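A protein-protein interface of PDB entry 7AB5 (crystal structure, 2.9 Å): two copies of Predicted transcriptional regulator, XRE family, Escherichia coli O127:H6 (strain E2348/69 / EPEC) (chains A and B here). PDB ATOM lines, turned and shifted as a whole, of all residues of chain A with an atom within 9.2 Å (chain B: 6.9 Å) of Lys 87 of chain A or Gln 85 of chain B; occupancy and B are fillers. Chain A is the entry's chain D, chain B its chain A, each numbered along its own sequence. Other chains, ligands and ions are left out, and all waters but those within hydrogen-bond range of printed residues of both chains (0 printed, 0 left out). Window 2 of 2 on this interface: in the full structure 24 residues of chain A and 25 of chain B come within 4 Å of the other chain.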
ATOM      1  N   ILE A  71       0.263  -1.822  35.598  1.00  0.00           N
ATOM      2  CA  ILE A  71       1.720  -1.821  35.561  1.00  0.00           C
ATOM      3  C   ILE A  71       2.238  -0.902  36.658  1.00  0.00           C
ATOM      4  O   ILE A  71       1.809   0.253  36.772  1.00  0.00           O
ATOM      5  CB  ILE A  71       2.227  -1.379  34.180  1.00  0.00           C
ATOM      6  CG1 ILE A  71       1.462  -2.110  33.077  1.00  0.00           C
ATOM      7  CG2 ILE A  71       3.720  -1.627  34.055  1.00  0.00           C
ATOM      8  CD1 ILE A  71       1.784  -1.614  31.691  1.00  0.00           C
ATOM      9  N   THR A  75       7.963   0.004  36.968  1.00  0.00           N
ATOM     10  CA  THR A  75       8.043  -0.597  35.641  1.00  0.00           C
ATOM     11  C   THR A  75       7.696   0.411  34.548  1.00  0.00           C
ATOM     12  O   THR A  75       8.164   0.276  33.412  1.00  0.00           O
ATOM     13  CB  THR A  75       7.118  -1.816  35.561  1.00  0.00           C
ATOM     14  OG1 THR A  75       7.475  -2.756  36.581  1.00  0.00           O
ATOM     15  CG2 THR A  75       7.238  -2.505  34.208  1.00  0.00           C
ATOM     16  N   ARG A  78      10.561   2.503  33.942  1.00  0.00           N
ATOM     17  CA  ARG A  78      11.444   1.626  33.172  1.00  0.00           C
ATOM     18  C   ARG A  78      11.076   1.692  31.702  1.00  0.00           C
ATOM     19  O   ARG A  78      11.927   1.948  30.851  1.00  0.00           O
ATOM     20  CB  ARG A  78      11.393   0.157  33.656  1.00  0.00           C
ATOM     21  CG  ARG A  78      12.676  -0.607  33.369  1.00  0.00           C
ATOM     22  CD  ARG A  78      13.732   0.399  33.771  1.00  0.00           C
ATOM     23  NE  ARG A  78      13.854   0.127  35.199  1.00  0.00           N
ATOM     24  CZ  ARG A  78      14.676  -0.752  35.754  1.00  0.00           C
ATOM     25  NH1 ARG A  78      15.800  -1.145  35.141  1.00  0.00           N
ATOM     26  NH2 ARG A  78      14.384  -1.211  36.967  1.00  0.00           N
ATOM     27  N   LEU A  79       9.784   1.536  31.398  1.00  0.00           N
ATOM     28  CA  LEU A  79       9.356   1.419  30.006  1.00  0.00           C
ATOM     29  C   LEU A  79       9.660   2.690  29.224  1.00  0.00           C
ATOM     30  O   LEU A  79      10.118   2.634  28.077  1.00  0.00           O
ATOM     31  CB  LEU A  79       7.861   1.093  29.965  1.00  0.00           C
ATOM     32  CG  LEU A  79       7.072   0.619  28.746  1.00  0.00           C
ATOM     33  CD1 LEU A  79       5.706   0.239  29.255  1.00  0.00           C
ATOM     34  CD2 LEU A  79       6.940   1.694  27.677  1.00  0.00           C
ATOM     35  N   ASP A  82      14.012   2.818  28.715  1.00  0.00           N
ATOM     36  CA  ASP A  82      14.337   1.712  27.814  1.00  0.00           C
ATOM     37  C   ASP A  82      13.444   0.511  28.098  1.00  0.00           C
ATOM     38  O   ASP A  82      13.619  -0.168  29.118  1.00  0.00           O
ATOM     39  CB  ASP A  82      15.810   1.311  27.923  1.00  0.00           C
ATOM     40  CG  ASP A  82      16.274   0.476  26.739  1.00  0.00           C
ATOM     41  OD1 ASP A  82      15.583   0.488  25.701  1.00  0.00           O
ATOM     42  OD2 ASP A  82      17.328  -0.188  26.835  1.00  0.00           O
ATOM     43  N   PRO A  83      12.491   0.211  27.213  1.00  0.00           N
ATOM     44  CA  PRO A  83      11.590  -0.924  27.444  1.00  0.00           C
ATOM     45  C   PRO A  83      12.167  -2.248  26.963  1.00  0.00           C
ATOM     46  O   PRO A  83      11.423  -3.207  26.731  1.00  0.00           O
ATOM     47  CB  PRO A  83      10.350  -0.533  26.637  1.00  0.00           C
ATOM     48  CG  PRO A  83      10.926   0.183  25.458  1.00  0.00           C
ATOM     49  CD  PRO A  83      12.133   0.949  25.988  1.00  0.00           C
ATOM     50  N   GLU A  84      13.493  -2.306  26.818  1.00  0.00           N
ATOM     51  CA  GLU A  84      14.133  -3.495  26.261  1.00  0.00           C
ATOM     52  C   GLU A  84      13.855  -4.730  27.109  1.00  0.00           C
ATOM     53  O   GLU A  84      13.656  -5.827  26.574  1.00  0.00           O
ATOM     54  CB  GLU A  84      15.638  -3.260  26.126  1.00  0.00           C
ATOM     55  CG  GLU A  84      16.431  -4.501  25.749  1.00  0.00           C
ATOM     56  CD  GLU A  84      16.775  -4.548  24.273  1.00  0.00           C
ATOM     57  OE1 GLU A  84      17.233  -5.611  23.802  1.00  0.00           O
ATOM     58  OE2 GLU A  84      16.589  -3.522  23.585  1.00  0.00           O
ATOM     59  N   GLN A  85      13.823  -4.572  28.430  1.00  0.00           N
ATOM     60  CA  GLN A  85      13.605  -5.686  29.342  1.00  0.00           C
ATOM     61  C   GLN A  85      12.169  -5.767  29.843  1.00  0.00           C
ATOM     62  O   GLN A  85      11.898  -6.499  30.799  1.00  0.00           O
ATOM     63  CB  GLN A  85      14.567  -5.584  30.530  1.00  0.00           C
ATOM     64  CG  GLN A  85      16.032  -5.490  30.131  1.00  0.00           C
ATOM     65  CD  GLN A  85      16.490  -6.670  29.293  1.00  0.00           C
ATOM     66  OE1 GLN A  85      16.011  -7.791  29.463  1.00  0.00           O
ATOM     67  NE2 GLN A  85      17.419  -6.420  28.378  1.00  0.00           N
ATOM     68  N   VAL A  86      11.246  -5.039  29.217  1.00  0.00           N
ATOM     69  CA  VAL A  86       9.851  -4.978  29.643  1.00  0.00           C
ATOM     70  C   VAL A  86       9.030  -5.923  28.777  1.00  0.00           C
ATOM     71  O   VAL A  86       9.252  -6.016  27.563  1.00  0.00           O
ATOM     72  CB  VAL A  86       9.319  -3.533  29.554  1.00  0.00           C
ATOM     73  CG1 VAL A  86       7.830  -3.480  29.860  1.00  0.00           C
ATOM     74  CG2 VAL A  86      10.097  -2.626  30.498  1.00  0.00           C
ATOM     75  N   LYS A  87       8.091  -6.638  29.404  1.00  0.00           N
ATOM     76  CA  LYS A  87       7.199  -7.530  28.671  1.00  0.00           C
ATOM     77  C   LYS A  87       6.540  -6.796  27.511  1.00  0.00           C
ATOM     78  O   LYS A  87       6.128  -5.641  27.641  1.00  0.00           O
ATOM     79  CB  LYS A  87       6.114  -8.096  29.591  1.00  0.00           C
ATOM     80  CG  LYS A  87       6.590  -8.594  30.940  1.00  0.00           C
ATOM     81  CD  LYS A  87       5.398  -9.003  31.797  1.00  0.00           C
ATOM     82  CE  LYS A  87       5.766 -10.074  32.812  1.00  0.00           C
ATOM     83  NZ  LYS A  87       6.739 -11.058  32.260  1.00  0.00           N
ATOM     84  N   PHE A  88       6.443  -7.481  26.370  1.00  0.00           N
ATOM     85  CA  PHE A  88       5.826  -6.871  25.196  1.00  0.00           C
ATOM     86  C   PHE A  88       4.377  -6.488  25.466  1.00  0.00           C
ATOM     87  O   PHE A  88       3.897  -5.462  24.969  1.00  0.00           O
ATOM     88  CB  PHE A  88       5.910  -7.816  23.999  1.00  0.00           C
ATOM     89  CG  PHE A  88       5.244  -7.282  22.765  1.00  0.00           C
ATOM     90  CD1 PHE A  88       5.938  -6.473  21.882  1.00  0.00           C
ATOM     91  CD2 PHE A  88       3.919  -7.580  22.492  1.00  0.00           C
ATOM     92  CE1 PHE A  88       5.324  -5.975  20.749  1.00  0.00           C
ATOM     93  CE2 PHE A  88       3.300  -7.083  21.364  1.00  0.00           C
ATOM     94  CZ  PHE A  88       4.002  -6.279  20.492  1.00  0.00           C
ATOM     95  N   GLY A  89       3.662  -7.305  26.242  1.00  0.00           N
ATOM     96  CA  GLY A  89       2.261  -7.021  26.506  1.00  0.00           C
ATOM     97  C   GLY A  89       2.052  -5.697  27.215  1.00  0.00           C
ATOM     98  O   GLY A  89       1.064  -5.001  26.970  1.00  0.00           O
ATOM     99  N   SER A  90       2.983  -5.327  28.098  1.00  0.00           N
ATOM    100  CA  SER A  90       2.866  -4.061  28.815  1.00  0.00           C
ATOM    101  C   SER A  90       3.109  -2.877  27.889  1.00  0.00           C
ATOM    102  O   SER A  90       2.366  -1.889  27.922  1.00  0.00           O
ATOM    103  CB  SER A  90       3.841  -4.037  29.993  1.00  0.00           C
ATOM    104  OG  SER A  90       3.572  -5.097  30.893  1.00  0.00           O
ATOM    105  N   VAL A  91       4.154  -2.952  27.060  1.00  0.00           N
ATOM    106  CA  VAL A  91       4.404  -1.899  26.079  1.00  0.00           C
ATOM    107  C   VAL A  91       3.206  -1.753  25.149  1.00  0.00           C
ATOM    108  O   VAL A  91       2.740  -0.642  24.874  1.00  0.00           O
ATOM    109  CB  VAL A  91       5.695  -2.189  25.294  1.00  0.00           C
ATOM    110  CG1 VAL A  91       5.922  -1.118  24.236  1.00  0.00           C
ATOM    111  CG2 VAL A  91       6.882  -2.269  26.240  1.00  0.00           C
ATOM    112  N   PHE A  92       2.685  -2.881  24.660  1.00  0.00           N
ATOM    113  CA  PHE A  92       1.494  -2.839  23.820  1.00  0.00           C
ATOM    114  C   PHE A  92       0.297  -2.281  24.579  1.00  0.00           C
ATOM    115  O   PHE A  92      -0.545  -1.594  23.989  1.00  0.00           O
ATOM    116  CB  PHE A  92       1.178  -4.235  23.284  1.00  0.00           C
ATOM    117  CG  PHE A  92       0.109  -4.249  22.233  1.00  0.00           C
ATOM    118  CD1 PHE A  92       0.416  -3.973  20.911  1.00  0.00           C
ATOM    119  CD2 PHE A  92      -1.206  -4.527  22.566  1.00  0.00           C
ATOM    120  CE1 PHE A  92      -0.568  -3.981  19.940  1.00  0.00           C
ATOM    121  CE2 PHE A  92      -2.193  -4.536  21.600  1.00  0.00           C
ATOM    122  CZ  PHE A  92      -1.873  -4.262  20.286  1.00  0.00           C
ATOM    123  N   ALA A  93       0.205  -2.562  25.881  1.00  0.00           N
ATOM    124  CA  ALA A  93      -0.897  -2.031  26.676  1.00  0.00           C
ATOM    125  C   ALA A  93      -0.761  -0.528  26.878  1.00  0.00           C
ATOM    126  O   ALA A  93      -1.748   0.211  26.775  1.00  0.00           O
ATOM    127  CB  ALA A  93      -0.968  -2.748  28.023  1.00  0.00           C
ATOM    128  N   VAL A  94       0.453  -0.056  27.171  1.00  0.00           N
ATOM    129  CA  VAL A  94       0.666   1.372  27.387  1.00  0.00           C
ATOM    130  C   VAL A  94       0.431   2.149  26.097  1.00  0.00           C
ATOM    131  O   VAL A  94      -0.102   3.265  26.116  1.00  0.00           O
ATOM    132  CB  VAL A  94       2.076   1.613  27.959  1.00  0.00           C
ATOM    133  CG1 VAL A  94       2.480   3.071  27.819  1.00  0.00           C
ATOM    134  CG2 VAL A  94       2.126   1.191  29.416  1.00  0.00           C
ATOM    135  N   PRO B  44      -1.030  -8.628  20.801  1.00  0.00           N
ATOM    136  CA  PRO B  44       0.306  -9.248  20.778  1.00  0.00           C
ATOM    137  C   PRO B  44       0.330 -10.556  20.012  1.00  0.00           C
ATOM    138  O   PRO B  44       1.300 -10.836  19.296  1.00  0.00           O
ATOM    139  CB  PRO B  44       0.619  -9.446  22.269  1.00  0.00           C
ATOM    140  CG  PRO B  44      -0.161  -8.377  22.949  1.00  0.00           C
ATOM    141  CD  PRO B  44      -1.439  -8.263  22.169  1.00  0.00           C
ATOM    142  N   ARG B  78       7.455 -19.479  22.025  1.00  0.00           N
ATOM    143  CA  ARG B  78       6.489 -18.647  22.735  1.00  0.00           C
ATOM    144  C   ARG B  78       6.300 -17.311  22.031  1.00  0.00           C
ATOM    145  O   ARG B  78       5.188 -16.768  22.005  1.00  0.00           O
ATOM    146  CB  ARG B  78       6.935 -18.422  24.178  1.00  0.00           C
ATOM    147  CG  ARG B  78       6.884 -19.655  25.062  1.00  0.00           C
ATOM    148  CD  ARG B  78       7.852 -19.522  26.226  1.00  0.00           C
ATOM    149  NE  ARG B  78       7.380 -18.558  27.213  1.00  0.00           N
ATOM    150  CZ  ARG B  78       6.370 -18.763  28.047  1.00  0.00           C
ATOM    151  NH1 ARG B  78       5.716 -19.914  28.076  1.00  0.00           N
ATOM    152  NH2 ARG B  78       6.011 -17.790  28.881  1.00  0.00           N
ATOM    153  N   ASP B  82       2.294 -16.413  21.380  1.00  0.00           N
ATOM    154  CA  ASP B  82       1.735 -15.223  22.021  1.00  0.00           C
ATOM    155  C   ASP B  82       2.867 -14.500  22.731  1.00  0.00           C
ATOM    156  O   ASP B  82       3.235 -14.858  23.859  1.00  0.00           O
ATOM    157  CB  ASP B  82       0.611 -15.565  22.995  1.00  0.00           C
ATOM    158  CG  ASP B  82      -0.282 -14.377  23.291  1.00  0.00           C
ATOM    159  OD1 ASP B  82      -0.661 -13.666  22.343  1.00  0.00           O
ATOM    160  OD2 ASP B  82      -0.610 -14.155  24.475  1.00  0.00           O
ATOM    161  N   PRO B  83       3.439 -13.467  22.108  1.00  0.00           N
ATOM    162  CA  PRO B  83       4.584 -12.782  22.721  1.00  0.00           C
ATOM    163  C   PRO B  83       4.193 -11.798  23.813  1.00  0.00           C
ATOM    164  O   PRO B  83       4.930 -10.844  24.074  1.00  0.00           O
ATOM    165  CB  PRO B  83       5.227 -12.061  21.531  1.00  0.00           C
ATOM    166  CG  PRO B  83       4.082 -11.766  20.631  1.00  0.00           C
ATOM    167  CD  PRO B  83       3.141 -12.945  20.763  1.00  0.00           C
ATOM    168  N   GLU B  84       3.044 -12.020  24.458  1.00  0.00           N
ATOM    169  CA  GLU B  84       2.606 -11.123  25.525  1.00  0.00           C
ATOM    170  C   GLU B  84       3.591 -11.099  26.686  1.00  0.00           C
ATOM    171  O   GLU B  84       3.779 -10.053  27.317  1.00  0.00           O
ATOM    172  CB  GLU B  84       1.221 -11.535  26.022  1.00  0.00           C
ATOM    173  CG  GLU B  84       0.632 -10.598  27.068  1.00  0.00           C
ATOM    174  CD  GLU B  84      -0.775 -10.146  26.730  1.00  0.00           C
ATOM    175  OE1 GLU B  84      -1.632 -11.015  26.466  1.00  0.00           O
ATOM    176  OE2 GLU B  84      -1.024  -8.921  26.733  1.00  0.00           O
ATOM    177  N   GLN B  85       4.233 -12.229  26.976  1.00  0.00           N
ATOM    178  CA  GLN B  85       5.109 -12.361  28.132  1.00  0.00           C
ATOM    179  C   GLN B  85       6.587 -12.336  27.767  1.00  0.00           C
ATOM    180  O   GLN B  85       7.431 -12.587  28.633  1.00  0.00           O
ATOM    181  CB  GLN B  85       4.784 -13.652  28.885  1.00  0.00           C
ATOM    182  CG  GLN B  85       3.397 -13.660  29.495  1.00  0.00           C
ATOM    183  CD  GLN B  85       3.346 -12.925  30.817  1.00  0.00           C
ATOM    184  OE1 GLN B  85       2.594 -11.965  30.976  1.00  0.00           O
ATOM    185  NE2 GLN B  85       4.142 -13.379  31.779  1.00  0.00           N
ATOM    186  N   VAL B  86       6.921 -12.039  26.514  1.00  0.00           N
ATOM    187  CA  VAL B  86       8.304 -12.001  26.054  1.00  0.00           C
ATOM    188  C   VAL B  86       8.816 -10.572  26.148  1.00  0.00           C
ATOM    189  O   VAL B  86       8.078  -9.615  25.874  1.00  0.00           O
ATOM    190  CB  VAL B  86       8.428 -12.544  24.618  1.00  0.00           C
ATOM    191  CG1 VAL B  86       9.882 -12.826  24.279  1.00  0.00           C
ATOM    192  CG2 VAL B  86       7.593 -13.802  24.459  1.00  0.00           C
ATOM    193  N   LYS B  87      10.078 -10.427  26.550  1.00  0.00           N
ATOM    194  CA  LYS B  87      10.713  -9.116  26.618  1.00  0.00           C
ATOM    195  C   LYS B  87      10.595  -8.398  25.281  1.00  0.00           C
ATOM    196  O   LYS B  87      10.843  -8.986  24.224  1.00  0.00           O
ATOM    197  CB  LYS B  87      12.183  -9.271  27.013  1.00  0.00           C
ATOM    198  CG  LYS B  87      12.396  -9.943  28.362  1.00  0.00           C
ATOM    199  CD  LYS B  87      13.872 -10.026  28.713  1.00  0.00           C
ATOM    200  CE  LYS B  87      14.085 -10.671  30.075  1.00  0.00           C
ATOM    201  NZ  LYS B  87      14.063 -12.160  30.010  1.00  0.00           N
ATOM    202  N   PHE B  88      10.198  -7.123  25.334  1.00  0.00           N
ATOM    203  CA  PHE B  88       9.977  -6.364  24.107  1.00  0.00           C
ATOM    204  C   PHE B  88      11.230  -6.327  23.242  1.00  0.00           C
ATOM    205  O   PHE B  88      11.141  -6.347  22.008  1.00  0.00           O
ATOM    206  CB  PHE B  88       9.518  -4.944  24.438  1.00  0.00           C
ATOM    207  CG  PHE B  88       9.468  -4.035  23.245  1.00  0.00           C
ATOM    208  CD1 PHE B  88       8.374  -4.043  22.397  1.00  0.00           C
ATOM    209  CD2 PHE B  88      10.520  -3.176  22.966  1.00  0.00           C
ATOM    210  CE1 PHE B  88       8.328  -3.210  21.294  1.00  0.00           C
ATOM    211  CE2 PHE B  88      10.478  -2.342  21.863  1.00  0.00           C
ATOM    212  CZ  PHE B  88       9.383  -2.360  21.027  1.00  0.00           C
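N of Phe 88 of chain A is in hydrogen-bond range of O of Val 86 of chain B, at 2.7 Å. The backbone carbonyl oxygen (O) of Glu 84 of chain B sits at hydrogen-bond distance from the backbone NH (N) of Gly 89 of chain A (3.0 Å). The backbone NH (N) of Phe 88 of chain B sits at hydrogen-bond distance from the backbone carbonyl oxygen (O) of Val 86 of chain A, 2.7 Å away.
Among the printed residues, merely in contact across the chains: Pro 83 of chain A with Phe 88 of chain B (3.5 Å), Glu 84 of chain A with Lys 87 of chain B (3.8 Å), Glu 84 of chain A with Phe 88 of chain B (3.9 Å), Gln 85 of chain A with Lys 87 of chain B (3.2 Å), Val 86 of chain A with Lys 87 of chain B (3.6 Å), Lys 87 of chain A with Glu 84 of chain B (3.8 Å), Lys 87 of chain A with Gln 85 of chain B (3.5 Å), Lys 87 of chain A with Val 86 of chain B (3.6 Å), Phe 88 of chain A with Pro 44 of chain B (3.7 Å), Phe 88 of chain A with Pro 83 of chain B (3.2 Å), Phe 88 of chain A with Glu 84 of chain B (3.8 Å), Phe 88 of chain A with Phe 88 of chain B (3.5 Å) and Phe 92 of chain A with Pro 44 of chain B (3.8 Å).
Of chain B, only Glu 84 (3.8 Å), Gln 85 (3.5 Å) and Val 86 (3.6 Å) come within 4 Å of Lys 87 of chain A. Val 91 of chain A touches none of the printed residues of chain B. Of the printed residues of chain A, Pro 83 of chain B touches Phe 88 (3.2 Å). Of the printed residues of chain A, Glu 84 of chain B touches Lys 87 (3.8 Å), Phe 88 (3.8 Å) and Gly 89 (3.0 Å). Printed residues of chain A within 4 Å of Gln 85 of chain B: Lys 87. Val 86 of chain B touches just these residues of chain A: Lys 87 and Phe 88. The nearest residue of chain B that does not touch Lys 87 of chain A is Phe 88 of chain B (4.3 Å). The nearest residue of chain A that does not touch Gln 85 of chain B is Gly 89 of chain A (5.0 Å).
Of the 17 printed residues of chain A, 8 touch a printed residue of chain B. Hydrophobic or aromatic side chains of chain B that line the printed part of chain A: Pro 44 and Phe 88. Among the printed residues, 16 pairs touch across the chains.
Pro 83 of chain A touches Phe 88 of chain B, and with the chains exchanged Phe 88 of chain A touches Pro 83 of chain B. Glu 84 of chain A touches Phe 88 of chain B, and with the chains exchanged Phe 88 of chain A touches Glu 84 of chain B. Val 86 of chain A touches Phe 88 of chain B, and with the chains exchanged Phe 88 of chain A touches Val 86 of chain B. Phe 88 of chain B touches its own counterpart, Phe 88 of chain A. Positions printed for both chains: 78, 82, 83, 84, 85, 86, 87 and 88. Of the 16 pairs that touch across the chains among the printed residues, 13 have their exchanged pair printed and touching as well.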
